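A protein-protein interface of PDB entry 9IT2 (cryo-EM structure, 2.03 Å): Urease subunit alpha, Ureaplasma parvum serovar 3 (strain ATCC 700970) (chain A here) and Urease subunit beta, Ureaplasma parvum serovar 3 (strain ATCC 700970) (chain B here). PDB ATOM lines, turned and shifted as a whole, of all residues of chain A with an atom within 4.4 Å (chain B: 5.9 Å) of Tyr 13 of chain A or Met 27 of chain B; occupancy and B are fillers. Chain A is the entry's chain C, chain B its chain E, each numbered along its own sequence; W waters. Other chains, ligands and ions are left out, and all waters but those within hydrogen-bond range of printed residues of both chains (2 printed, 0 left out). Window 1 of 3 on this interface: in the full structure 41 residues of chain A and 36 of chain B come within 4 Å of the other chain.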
ATOM      1  N   MET A   1      11.147  14.413 -14.355  1.00  0.00           N
ATOM      2  CA  MET A   1       9.731  14.670 -14.130  1.00  0.00           C
ATOM      3  C   MET A   1       8.923  14.082 -15.282  1.00  0.00           C
ATOM      4  O   MET A   1       9.300  14.207 -16.446  1.00  0.00           O
ATOM      5  CB  MET A   1       9.483  16.180 -13.978  1.00  0.00           C
ATOM      6  CG  MET A   1       8.058  16.622 -13.604  1.00  0.00           C
ATOM      7  SD  MET A   1       6.724  16.259 -14.767  1.00  0.00           S
ATOM      8  CE  MET A   1       6.306  17.906 -15.332  1.00  0.00           C
ATOM      9  N   PHE A   2       7.809  13.437 -14.946  1.00  0.00           N
ATOM     10  CA  PHE A   2       6.902  12.876 -15.940  1.00  0.00           C
ATOM     11  C   PHE A   2       5.517  12.774 -15.312  1.00  0.00           C
ATOM     12  O   PHE A   2       5.302  13.182 -14.168  1.00  0.00           O
ATOM     13  CB  PHE A   2       7.399  11.520 -16.457  1.00  0.00           C
ATOM     14  CG  PHE A   2       7.546  10.471 -15.389  1.00  0.00           C
ATOM     15  CD1 PHE A   2       8.641  10.471 -14.538  1.00  0.00           C
ATOM     16  CD2 PHE A   2       6.593   9.477 -15.242  1.00  0.00           C
ATOM     17  CE1 PHE A   2       8.778   9.505 -13.561  1.00  0.00           C
ATOM     18  CE2 PHE A   2       6.724   8.509 -14.266  1.00  0.00           C
ATOM     19  CZ  PHE A   2       7.819   8.524 -13.425  1.00  0.00           C
ATOM     20  N   ILE A   4       1.783  10.279 -14.976  1.00  0.00           N
ATOM     21  CA  ILE A   4       1.227   8.933 -15.007  1.00  0.00           C
ATOM     22  C   ILE A   4      -0.268   9.016 -14.726  1.00  0.00           C
ATOM     23  O   ILE A   4      -0.720   9.870 -13.956  1.00  0.00           O
ATOM     24  CB  ILE A   4       1.938   8.004 -13.997  1.00  0.00           C
ATOM     25  CG1 ILE A   4       1.539   6.544 -14.224  1.00  0.00           C
ATOM     26  CG2 ILE A   4       1.657   8.435 -12.562  1.00  0.00           C
ATOM     27  CD1 ILE A   4       2.518   5.548 -13.644  1.00  0.00           C
ATOM     28  N   TYR A   9      -0.854   4.121 -11.951  1.00  0.00           N
ATOM     29  CA  TYR A   9      -0.317   4.336 -10.611  1.00  0.00           C
ATOM     30  C   TYR A   9      -0.915   3.349  -9.617  1.00  0.00           C
ATOM     31  O   TYR A   9      -0.197   2.791  -8.781  1.00  0.00           O
ATOM     32  CB  TYR A   9      -0.573   5.774 -10.162  1.00  0.00           C
ATOM     33  CG  TYR A   9       0.043   6.113  -8.819  1.00  0.00           C
ATOM     34  CD1 TYR A   9      -0.625   5.835  -7.631  1.00  0.00           C
ATOM     35  CD2 TYR A   9       1.295   6.708  -8.742  1.00  0.00           C
ATOM     36  CE1 TYR A   9      -0.061   6.140  -6.407  1.00  0.00           C
ATOM     37  CE2 TYR A   9       1.866   7.017  -7.524  1.00  0.00           C
ATOM     38  CZ  TYR A   9       1.185   6.731  -6.359  1.00  0.00           C
ATOM     39  OH  TYR A   9       1.750   7.040  -5.144  1.00  0.00           O
ATOM     40  N   SER A  10      -2.233   3.136  -9.678  1.00  0.00           N
ATOM     41  CA  SER A  10      -2.870   2.169  -8.794  1.00  0.00           C
ATOM     42  C   SER A  10      -2.408   0.751  -9.092  1.00  0.00           C
ATOM     43  O   SER A  10      -2.291  -0.067  -8.172  1.00  0.00           O
ATOM     44  CB  SER A  10      -4.391   2.270  -8.906  1.00  0.00           C
ATOM     45  OG  SER A  10      -4.800   2.314 -10.260  1.00  0.00           O
ATOM     46  N   ASP A  11      -2.147   0.440 -10.363  1.00  0.00           N
ATOM     47  CA  ASP A  11      -1.571  -0.858 -10.697  1.00  0.00           C
ATOM     48  C   ASP A  11      -0.214  -1.037 -10.032  1.00  0.00           C
ATOM     49  O   ASP A  11       0.098  -2.117  -9.516  1.00  0.00           O
ATOM     50  CB  ASP A  11      -1.443  -1.004 -12.214  1.00  0.00           C
ATOM     51  CG  ASP A  11      -2.763  -1.321 -12.884  1.00  0.00           C
ATOM     52  OD1 ASP A  11      -3.609  -1.990 -12.253  1.00  0.00           O
ATOM     53  OD2 ASP A  11      -2.953  -0.905 -14.045  1.00  0.00           O
ATOM     54  N   LEU A  12       0.607   0.013 -10.037  1.00  0.00           N
ATOM     55  CA  LEU A  12       1.956  -0.095  -9.491  1.00  0.00           C
ATOM     56  C   LEU A  12       1.970  -0.118  -7.964  1.00  0.00           C
ATOM     57  O   LEU A  12       2.691  -0.923  -7.364  1.00  0.00           O
ATOM     58  CB  LEU A  12       2.821   1.053 -10.010  1.00  0.00           C
ATOM     59  CG  LEU A  12       3.231   0.986 -11.482  1.00  0.00           C
ATOM     60  CD1 LEU A  12       3.782   2.326 -11.943  1.00  0.00           C
ATOM     61  CD2 LEU A  12       4.245  -0.124 -11.704  1.00  0.00           C
ATOM     62  N   TYR A  13       1.186   0.747  -7.315  1.00  0.00           N
ATOM     63  CA  TYR A  13       1.308   0.935  -5.875  1.00  0.00           C
ATOM     64  C   TYR A  13      -0.017   1.000  -5.128  1.00  0.00           C
ATOM     65  O   TYR A  13      -0.002   1.239  -3.918  1.00  0.00           O
ATOM     66  CB  TYR A  13       2.094   2.222  -5.564  1.00  0.00           C
ATOM     67  CG  TYR A  13       3.153   2.591  -6.576  1.00  0.00           C
ATOM     68  CD1 TYR A  13       4.355   1.902  -6.636  1.00  0.00           C
ATOM     69  CD2 TYR A  13       2.952   3.638  -7.465  1.00  0.00           C
ATOM     70  CE1 TYR A  13       5.327   2.240  -7.558  1.00  0.00           C
ATOM     71  CE2 TYR A  13       3.918   3.985  -8.390  1.00  0.00           C
ATOM     72  CZ  TYR A  13       5.103   3.282  -8.432  1.00  0.00           C
ATOM     73  OH  TYR A  13       6.067   3.621  -9.351  1.00  0.00           O
ATOM     74  N   GLY A  14      -1.152   0.793  -5.788  1.00  0.00           N
ATOM     75  CA  GLY A  14      -2.439   0.996  -5.162  1.00  0.00           C
ATOM     76  C   GLY A  14      -2.941   2.420  -5.320  1.00  0.00           C
ATOM     77  O   GLY A  14      -2.236   3.323  -5.777  1.00  0.00           O
ATOM     78  N   TYR A  39       5.664  11.295  -4.671  1.00  0.00           N
ATOM     79  CA  TYR A  39       5.431  10.684  -5.972  1.00  0.00           C
ATOM     80  C   TYR A  39       6.745  10.510  -6.724  1.00  0.00           C
ATOM     81  O   TYR A  39       7.540  11.447  -6.837  1.00  0.00           O
ATOM     82  CB  TYR A  39       4.452  11.535  -6.781  1.00  0.00           C
ATOM     83  CG  TYR A  39       3.037  11.486  -6.251  1.00  0.00           C
ATOM     84  CD1 TYR A  39       2.473  10.286  -5.834  1.00  0.00           C
ATOM     85  CD2 TYR A  39       2.270  12.639  -6.155  1.00  0.00           C
ATOM     86  CE1 TYR A  39       1.182  10.235  -5.346  1.00  0.00           C
ATOM     87  CE2 TYR A  39       0.976  12.597  -5.668  1.00  0.00           C
ATOM     88  CZ  TYR A  39       0.438  11.393  -5.264  1.00  0.00           C
ATOM     89  OH  TYR A  39      -0.847  11.346  -4.777  1.00  0.00           O
ATOM     90  N   GLY A  40       6.966   9.305  -7.241  1.00  0.00           N
ATOM     91  CA  GLY A  40       8.219   8.955  -7.873  1.00  0.00           C
ATOM     92  C   GLY A  40       9.250   8.332  -6.957  1.00  0.00           C
ATOM     93  O   GLY A  40      10.316   7.929  -7.438  1.00  0.00           O
ATOM     94  N   GLU A  42       8.225   5.918  -4.394  1.00  0.00           N
ATOM     95  CA  GLU A  42       7.529   4.871  -3.658  1.00  0.00           C
ATOM     96  C   GLU A  42       8.452   3.687  -3.387  1.00  0.00           C
ATOM     97  O   GLU A  42       9.310   3.337  -4.201  1.00  0.00           O
ATOM     98  CB  GLU A  42       6.297   4.403  -4.434  1.00  0.00           C
ATOM     99  CG  GLU A  42       5.151   5.404  -4.460  1.00  0.00           C
ATOM    100  CD  GLU A  42       5.343   6.491  -5.501  1.00  0.00           C
ATOM    101  OE1 GLU A  42       6.326   6.415  -6.270  1.00  0.00           O
ATOM    102  OE2 GLU A  42       4.512   7.420  -5.552  1.00  0.00           O
ATOM    103  N   VAL A  44       8.990  -0.099  -3.178  1.00  0.00           N
ATOM    104  CA  VAL A  44       8.461  -1.354  -3.697  1.00  0.00           C
ATOM    105  C   VAL A  44       9.571  -2.392  -3.655  1.00  0.00           C
ATOM    106  O   VAL A  44      10.729  -2.088  -3.963  1.00  0.00           O
ATOM    107  CB  VAL A  44       7.911  -1.195  -5.132  1.00  0.00           C
ATOM    108  CG1 VAL A  44       7.368  -2.517  -5.648  1.00  0.00           C
ATOM    109  CG2 VAL A  44       6.834  -0.129  -5.176  1.00  0.00           C
ATOM    110  N   ASN A  79       2.987   0.946   1.102  1.00  0.00           N
ATOM    111  CA  ASN A  79       1.789   1.344   0.356  1.00  0.00           C
ATOM    112  C   ASN A  79       0.513   0.806   1.000  1.00  0.00           C
ATOM    113  O   ASN A  79      -0.413   0.368   0.316  1.00  0.00           O
ATOM    114  CB  ASN A  79       1.884   0.908  -1.108  1.00  0.00           C
ATOM    115  CG  ASN A  79       3.273   1.089  -1.682  1.00  0.00           C
ATOM    116  OD1 ASN A  79       3.766   2.209  -1.798  1.00  0.00           O
ATOM    117  ND2 ASN A  79       3.913  -0.014  -2.042  1.00  0.00           N
ATOM    118  N   LYS A  90      -3.209   6.670   2.753  1.00  0.00           N
ATOM    119  CA  LYS A  90      -2.142   5.825   2.234  1.00  0.00           C
ATOM    120  C   LYS A  90      -0.829   6.176   2.923  1.00  0.00           C
ATOM    121  O   LYS A  90      -0.452   7.351   2.983  1.00  0.00           O
ATOM    122  CB  LYS A  90      -2.003   6.005   0.721  1.00  0.00           C
ATOM    123  CG  LYS A  90      -1.217   4.910   0.026  1.00  0.00           C
ATOM    124  CD  LYS A  90      -2.110   3.746  -0.362  1.00  0.00           C
ATOM    125  CE  LYS A  90      -1.430   2.851  -1.385  1.00  0.00           C
ATOM    126  NZ  LYS A  90      -1.155   3.564  -2.662  1.00  0.00           N
ATOM    127  N   GLU A 129       0.483  -2.858  -1.121  1.00  0.00           N
ATOM    128  CA  GLU A 129      -0.166  -2.128  -2.200  1.00  0.00           C
ATOM    129  C   GLU A 129      -1.465  -2.817  -2.603  1.00  0.00           C
ATOM    130  O   GLU A 129      -1.505  -4.037  -2.785  1.00  0.00           O
ATOM    131  CB  GLU A 129       0.771  -2.014  -3.404  1.00  0.00           C
ATOM    132  CG  GLU A 129       1.736  -3.183  -3.569  1.00  0.00           C
ATOM    133  CD  GLU A 129       3.077  -2.940  -2.898  1.00  0.00           C
ATOM    134  OE1 GLU A 129       3.097  -2.381  -1.782  1.00  0.00           O
ATOM    135  OE2 GLU A 129       4.114  -3.308  -3.487  1.00  0.00           O
ATOM    136  N   GLY A 130      -2.528  -2.030  -2.735  1.00  0.00           N
ATOM    137  CA  GLY A 130      -3.819  -2.561  -3.115  1.00  0.00           C
ATOM    138  C   GLY A 130      -4.587  -3.260  -2.016  1.00  0.00           C
ATOM    139  O   GLY A 130      -5.626  -3.861  -2.303  1.00  0.00           O
ATOM    140  N   ILE B  25      -1.127  12.263 -12.302  1.00  0.00           N
ATOM    141  CA  ILE B  25      -0.188  12.326 -11.189  1.00  0.00           C
ATOM    142  C   ILE B  25       1.185  12.694 -11.730  1.00  0.00           C
ATOM    143  O   ILE B  25       1.681  12.061 -12.670  1.00  0.00           O
ATOM    144  CB  ILE B  25      -0.141  10.996 -10.417  1.00  0.00           C
ATOM    145  CG1 ILE B  25      -1.562  10.495 -10.153  1.00  0.00           C
ATOM    146  CG2 ILE B  25       0.633  11.158  -9.117  1.00  0.00           C
ATOM    147  CD1 ILE B  25      -1.621   9.127  -9.536  1.00  0.00           C
ATOM    148  N   VAL B  26       1.794  13.716 -11.139  1.00  0.00           N
ATOM    149  CA  VAL B  26       3.116  14.182 -11.541  1.00  0.00           C
ATOM    150  C   VAL B  26       4.146  13.510 -10.642  1.00  0.00           C
ATOM    151  O   VAL B  26       4.194  13.764  -9.436  1.00  0.00           O
ATOM    152  CB  VAL B  26       3.219  15.709 -11.463  1.00  0.00           C
ATOM    153  CG1 VAL B  26       4.610  16.166 -11.869  1.00  0.00           C
ATOM    154  CG2 VAL B  26       2.160  16.358 -12.342  1.00  0.00           C
ATOM    155  N   MET B  27       4.976  12.650 -11.228  1.00  0.00           N
ATOM    156  CA  MET B  27       6.020  11.956 -10.490  1.00  0.00           C
ATOM    157  C   MET B  27       7.333  12.720 -10.584  1.00  0.00           C
ATOM    158  O   MET B  27       7.645  13.316 -11.619  1.00  0.00           O
ATOM    159  CB  MET B  27       6.206  10.535 -11.022  1.00  0.00           C
ATOM    160  CG  MET B  27       4.911   9.830 -11.378  1.00  0.00           C
ATOM    161  SD  MET B  27       4.049   9.220  -9.918  1.00  0.00           S
ATOM    162  CE  MET B  27       4.679   7.546  -9.832  1.00  0.00           C
ATOM    163  N   ASN B  28       8.101  12.688  -9.495  1.00  0.00           N
ATOM    164  CA  ASN B  28       9.386  13.383  -9.402  1.00  0.00           C
ATOM    165  C   ASN B  28       9.239  14.856  -9.774  1.00  0.00           C
ATOM    166  O   ASN B  28       9.992  15.402 -10.584  1.00  0.00           O
ATOM    167  CB  ASN B  28      10.443  12.697 -10.269  1.00  0.00           C
ATOM    168  CG  ASN B  28      10.686  11.259  -9.862  1.00  0.00           C
ATOM    169  OD1 ASN B  28      10.956  10.969  -8.697  1.00  0.00           O
ATOM    170  ND2 ASN B  28      10.592  10.349 -10.823  1.00  0.00           N
ATOM    171  N   GLU B  29       8.238  15.500  -9.177  1.00  0.00           N
ATOM    172  CA  GLU B  29       7.998  16.913  -9.429  1.00  0.00           C
ATOM    173  C   GLU B  29       9.160  17.745  -8.901  1.00  0.00           C
ATOM    174  O   GLU B  29       9.641  17.524  -7.785  1.00  0.00           O
ATOM    175  CB  GLU B  29       6.687  17.351  -8.777  1.00  0.00           C
ATOM    176  CG  GLU B  29       6.466  18.854  -8.758  1.00  0.00           C
ATOM    177  CD  GLU B  29       5.031  19.228  -8.447  1.00  0.00           C
ATOM    178  OE1 GLU B  29       4.140  18.372  -8.625  1.00  0.00           O
ATOM    179  OE2 GLU B  29       4.793  20.381  -8.025  1.00  0.00           O
ATOM    180  N   ASP B  83      14.601   8.448 -14.636  1.00  0.00           N
ATOM    181  CA  ASP B  83      13.381   9.200 -14.350  1.00  0.00           C
ATOM    182  C   ASP B  83      12.168   8.389 -14.806  1.00  0.00           C
ATOM    183  O   ASP B  83      11.431   8.753 -15.723  1.00  0.00           O
ATOM    184  CB  ASP B  83      13.432  10.568 -15.023  1.00  0.00           C
ATOM    185  CG  ASP B  83      12.336  11.497 -14.542  1.00  0.00           C
ATOM    186  OD1 ASP B  83      11.875  11.330 -13.394  1.00  0.00           O
ATOM    187  OD2 ASP B  83      11.934  12.393 -15.311  1.00  0.00           O
ATOM    188  N   PRO B  85       8.967   5.421 -13.254  1.00  0.00           N
ATOM    189  CA  PRO B  85       8.229   5.079 -12.033  1.00  0.00           C
ATOM    190  C   PRO B  85       9.036   4.154 -11.132  1.00  0.00           C
ATOM    191  O   PRO B  85       9.714   3.236 -11.599  1.00  0.00           O
ATOM    192  CB  PRO B  85       6.967   4.390 -12.562  1.00  0.00           C
ATOM    193  CG  PRO B  85       6.768   4.976 -13.908  1.00  0.00           C
ATOM    194  CD  PRO B  85       8.147   5.201 -14.462  1.00  0.00           C
ATOM    195  N   SER B  86       8.968   4.425  -9.830  1.00  0.00           N
ATOM    196  CA  SER B  86       9.739   3.662  -8.856  1.00  0.00           C
ATOM    197  C   SER B  86       9.380   2.183  -8.925  1.00  0.00           C
ATOM    198  O   SER B  86       8.202   1.815  -8.945  1.00  0.00           O
ATOM    199  CB  SER B  86       9.490   4.203  -7.449  1.00  0.00           C
ATOM    200  OG  SER B  86      10.242   3.488  -6.484  1.00  0.00           O
ATOM    201  N   GLY B  87      10.407   1.336  -8.963  1.00  0.00           N
ATOM    202  CA  GLY B  87      10.222  -0.093  -9.058  1.00  0.00           C
ATOM    203  C   GLY B  87      10.183  -0.644 -10.466  1.00  0.00           C
ATOM    204  O   GLY B  87      10.203  -1.870 -10.633  1.00  0.00           O
ATOM    205  N   THR B  88      10.126   0.213 -11.483  1.00  0.00           N
ATOM    206  CA  THR B  88      10.163  -0.237 -12.863  1.00  0.00           C
ATOM    207  C   THR B  88      11.613  -0.336 -13.336  1.00  0.00           C
ATOM    208  O   THR B  88      12.559  -0.120 -12.576  1.00  0.00           O
ATOM    209  CB  THR B  88       9.351   0.697 -13.761  1.00  0.00           C
ATOM    210  OG1 THR B  88       9.839   2.038 -13.628  1.00  0.00           O
ATOM    211  CG2 THR B  88       7.878   0.653 -13.384  1.00  0.00           C
HETATM  212  O   HOH W   1      11.159   7.427  -9.673  1.00  0.00           O
HETATM  213  O   HOH W   2       7.089  14.097  -6.672  1.00  0.00           O
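N of Ile 4 of chain A lies within hydrogen-bond range of O of Ile 25 of chain B.
The backbone carbonyl oxygen (O) of Phe 2 of chain A lies within hydrogen-bond range of the backbone NH (N) of Met 27 of chain B, at 3.0 Å.
The backbone NH of Asn 28 of chain B lies within hydrogen-bond range of the backbone carbonyl oxygen of Tyr 39 of chain A (3.0 Å).
O of Gly 40 of chain A sits close to OD1 of Asn 28 of chain B.
The side-chain carboxylate (OD1) of Asp 83 of chain B lies close to the backbone NH (N) of Met 1 of chain A.
O of Ser 86 of chain B lies within hydrogen-bond range of OH of Tyr 13 of chain A, 2.8 Å away.
The side-chain hydroxyl (OG) of Ser 86 of chain B lies within hydrogen-bond range of the backbone carbonyl oxygen (O) of Glu 42 of chain A (2.5 Å).
The side-chain amide nitrogen of Asn 28 of chain B lies within hydrogen-bond range of the side-chain carboxylate of Asp 83 of chain B (3.0 Å).
The side-chain hydroxyl of Tyr 9 of chain A lies within hydrogen-bond range of the side-chain carboxylate of Glu 42 of chain A, 2.8 Å away.
NZ of Lys 90 of chain A is in hydrogen-bond range of O of Tyr 13 of chain A (2.9 Å).
The backbone NH (N) of Gly 40 of chain A is in hydrogen-bond range of the side-chain carboxylate (OE1) of Glu 42 of chain A, at 3.1 Å.
Of chain B, only Met 27, Pro 85 and Ser 86 come within 4 Å of Tyr 13 of chain A.
Met 27 of chain B touches just these residues of chain A: Met 1, Phe 2, Ile 4, Tyr 9, Tyr 13, Tyr 39 and Gly 40.
Printed residues of chain A within 4 Å of Val 26 of chain B: Met 1 (3.6 Å), Phe 2 (3.6 Å) and Tyr 39 (3.5 Å).
Of the printed residues of chain B, Phe 2 of chain A touches Val 26, Met 27, Asn 28, Asp 83 and Pro 85.
Gly 14 of chain A touches none of the printed residues of chain B.
Gly 130 of chain A touches none of the printed residues of chain B.
The nearest residue of chain B that does not touch Tyr 13 of chain A is Gly 87 of chain B (4.9 Å).
The nearest printed residue of chain B that does not touch Ile 4 of chain A is Pro 85 of chain B (4.3 Å).
Of the 10 printed residues of chain B, 7 touch a printed residue of chain A.
Printed residues of chain B that touch a printed residue of chain A: Ile 25, Val 26, Met 27, Asn 28, Asp 83, Pro 85 and Ser 86.
Printed residues of chain A that touch a printed residue of chain B: Met 1, Phe 2, Ile 4, Tyr 9, Leu 12, Tyr 13, Tyr 39, Gly 40 and Glu 42.
Among the printed residues, pairs that only touch across the chains: Met 1 of chain A with Val 26 of chain B (3.6 Å), Met 1 of chain A with Met 27 of chain B (3.5 Å), Met 1 of chain A with Asn 28 of chain B (3.5 Å), Phe 2 of chain A with Val 26 of chain B (3.6 Å), Phe 2 of chain A with Asn 28 of chain B (3.4 Å), Phe 2 of chain A with Asp 83 of chain B (3.5 Å), Phe 2 of chain A with Pro 85 of chain B (3.3 Å), Ile 4 of chain A with Met 27 of chain B (3.7 Å), Tyr 9 of chain A with Ile 25 of chain B (3.5 Å), Tyr 9 of chain A with Met 27 of chain B (3.7 Å), Leu 12 of chain A with Pro 85 of chain B (3.8 Å), Tyr 13 of chain A with Met 27 of chain B (3.9 Å), Tyr 13 of chain A with Pro 85 of chain B (3.4 Å), Tyr 39 of chain A with Ile 25 of chain B (3.7 Å), Tyr 39 of chain A with Val 26 of chain B (3.5 Å), Tyr 39 of chain A with Met 27 of chain B (3.9 Å), Gly 40 of chain A with Met 27 of chain B (3.9 Å) and Gly 40 of chain A with Ser 86 of chain B (3.8 Å).
Water W1 lies within hydrogen-bond range of O of Gly 40 of chain A and ND2 of Asn 28 of chain B.
Water W2 lies within hydrogen-bond range of O of Tyr 39 of chain A (2.7 Å), N of Glu 29 of chain B (3.1 Å) and N of Asn 28 of chain B (3.3 Å).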
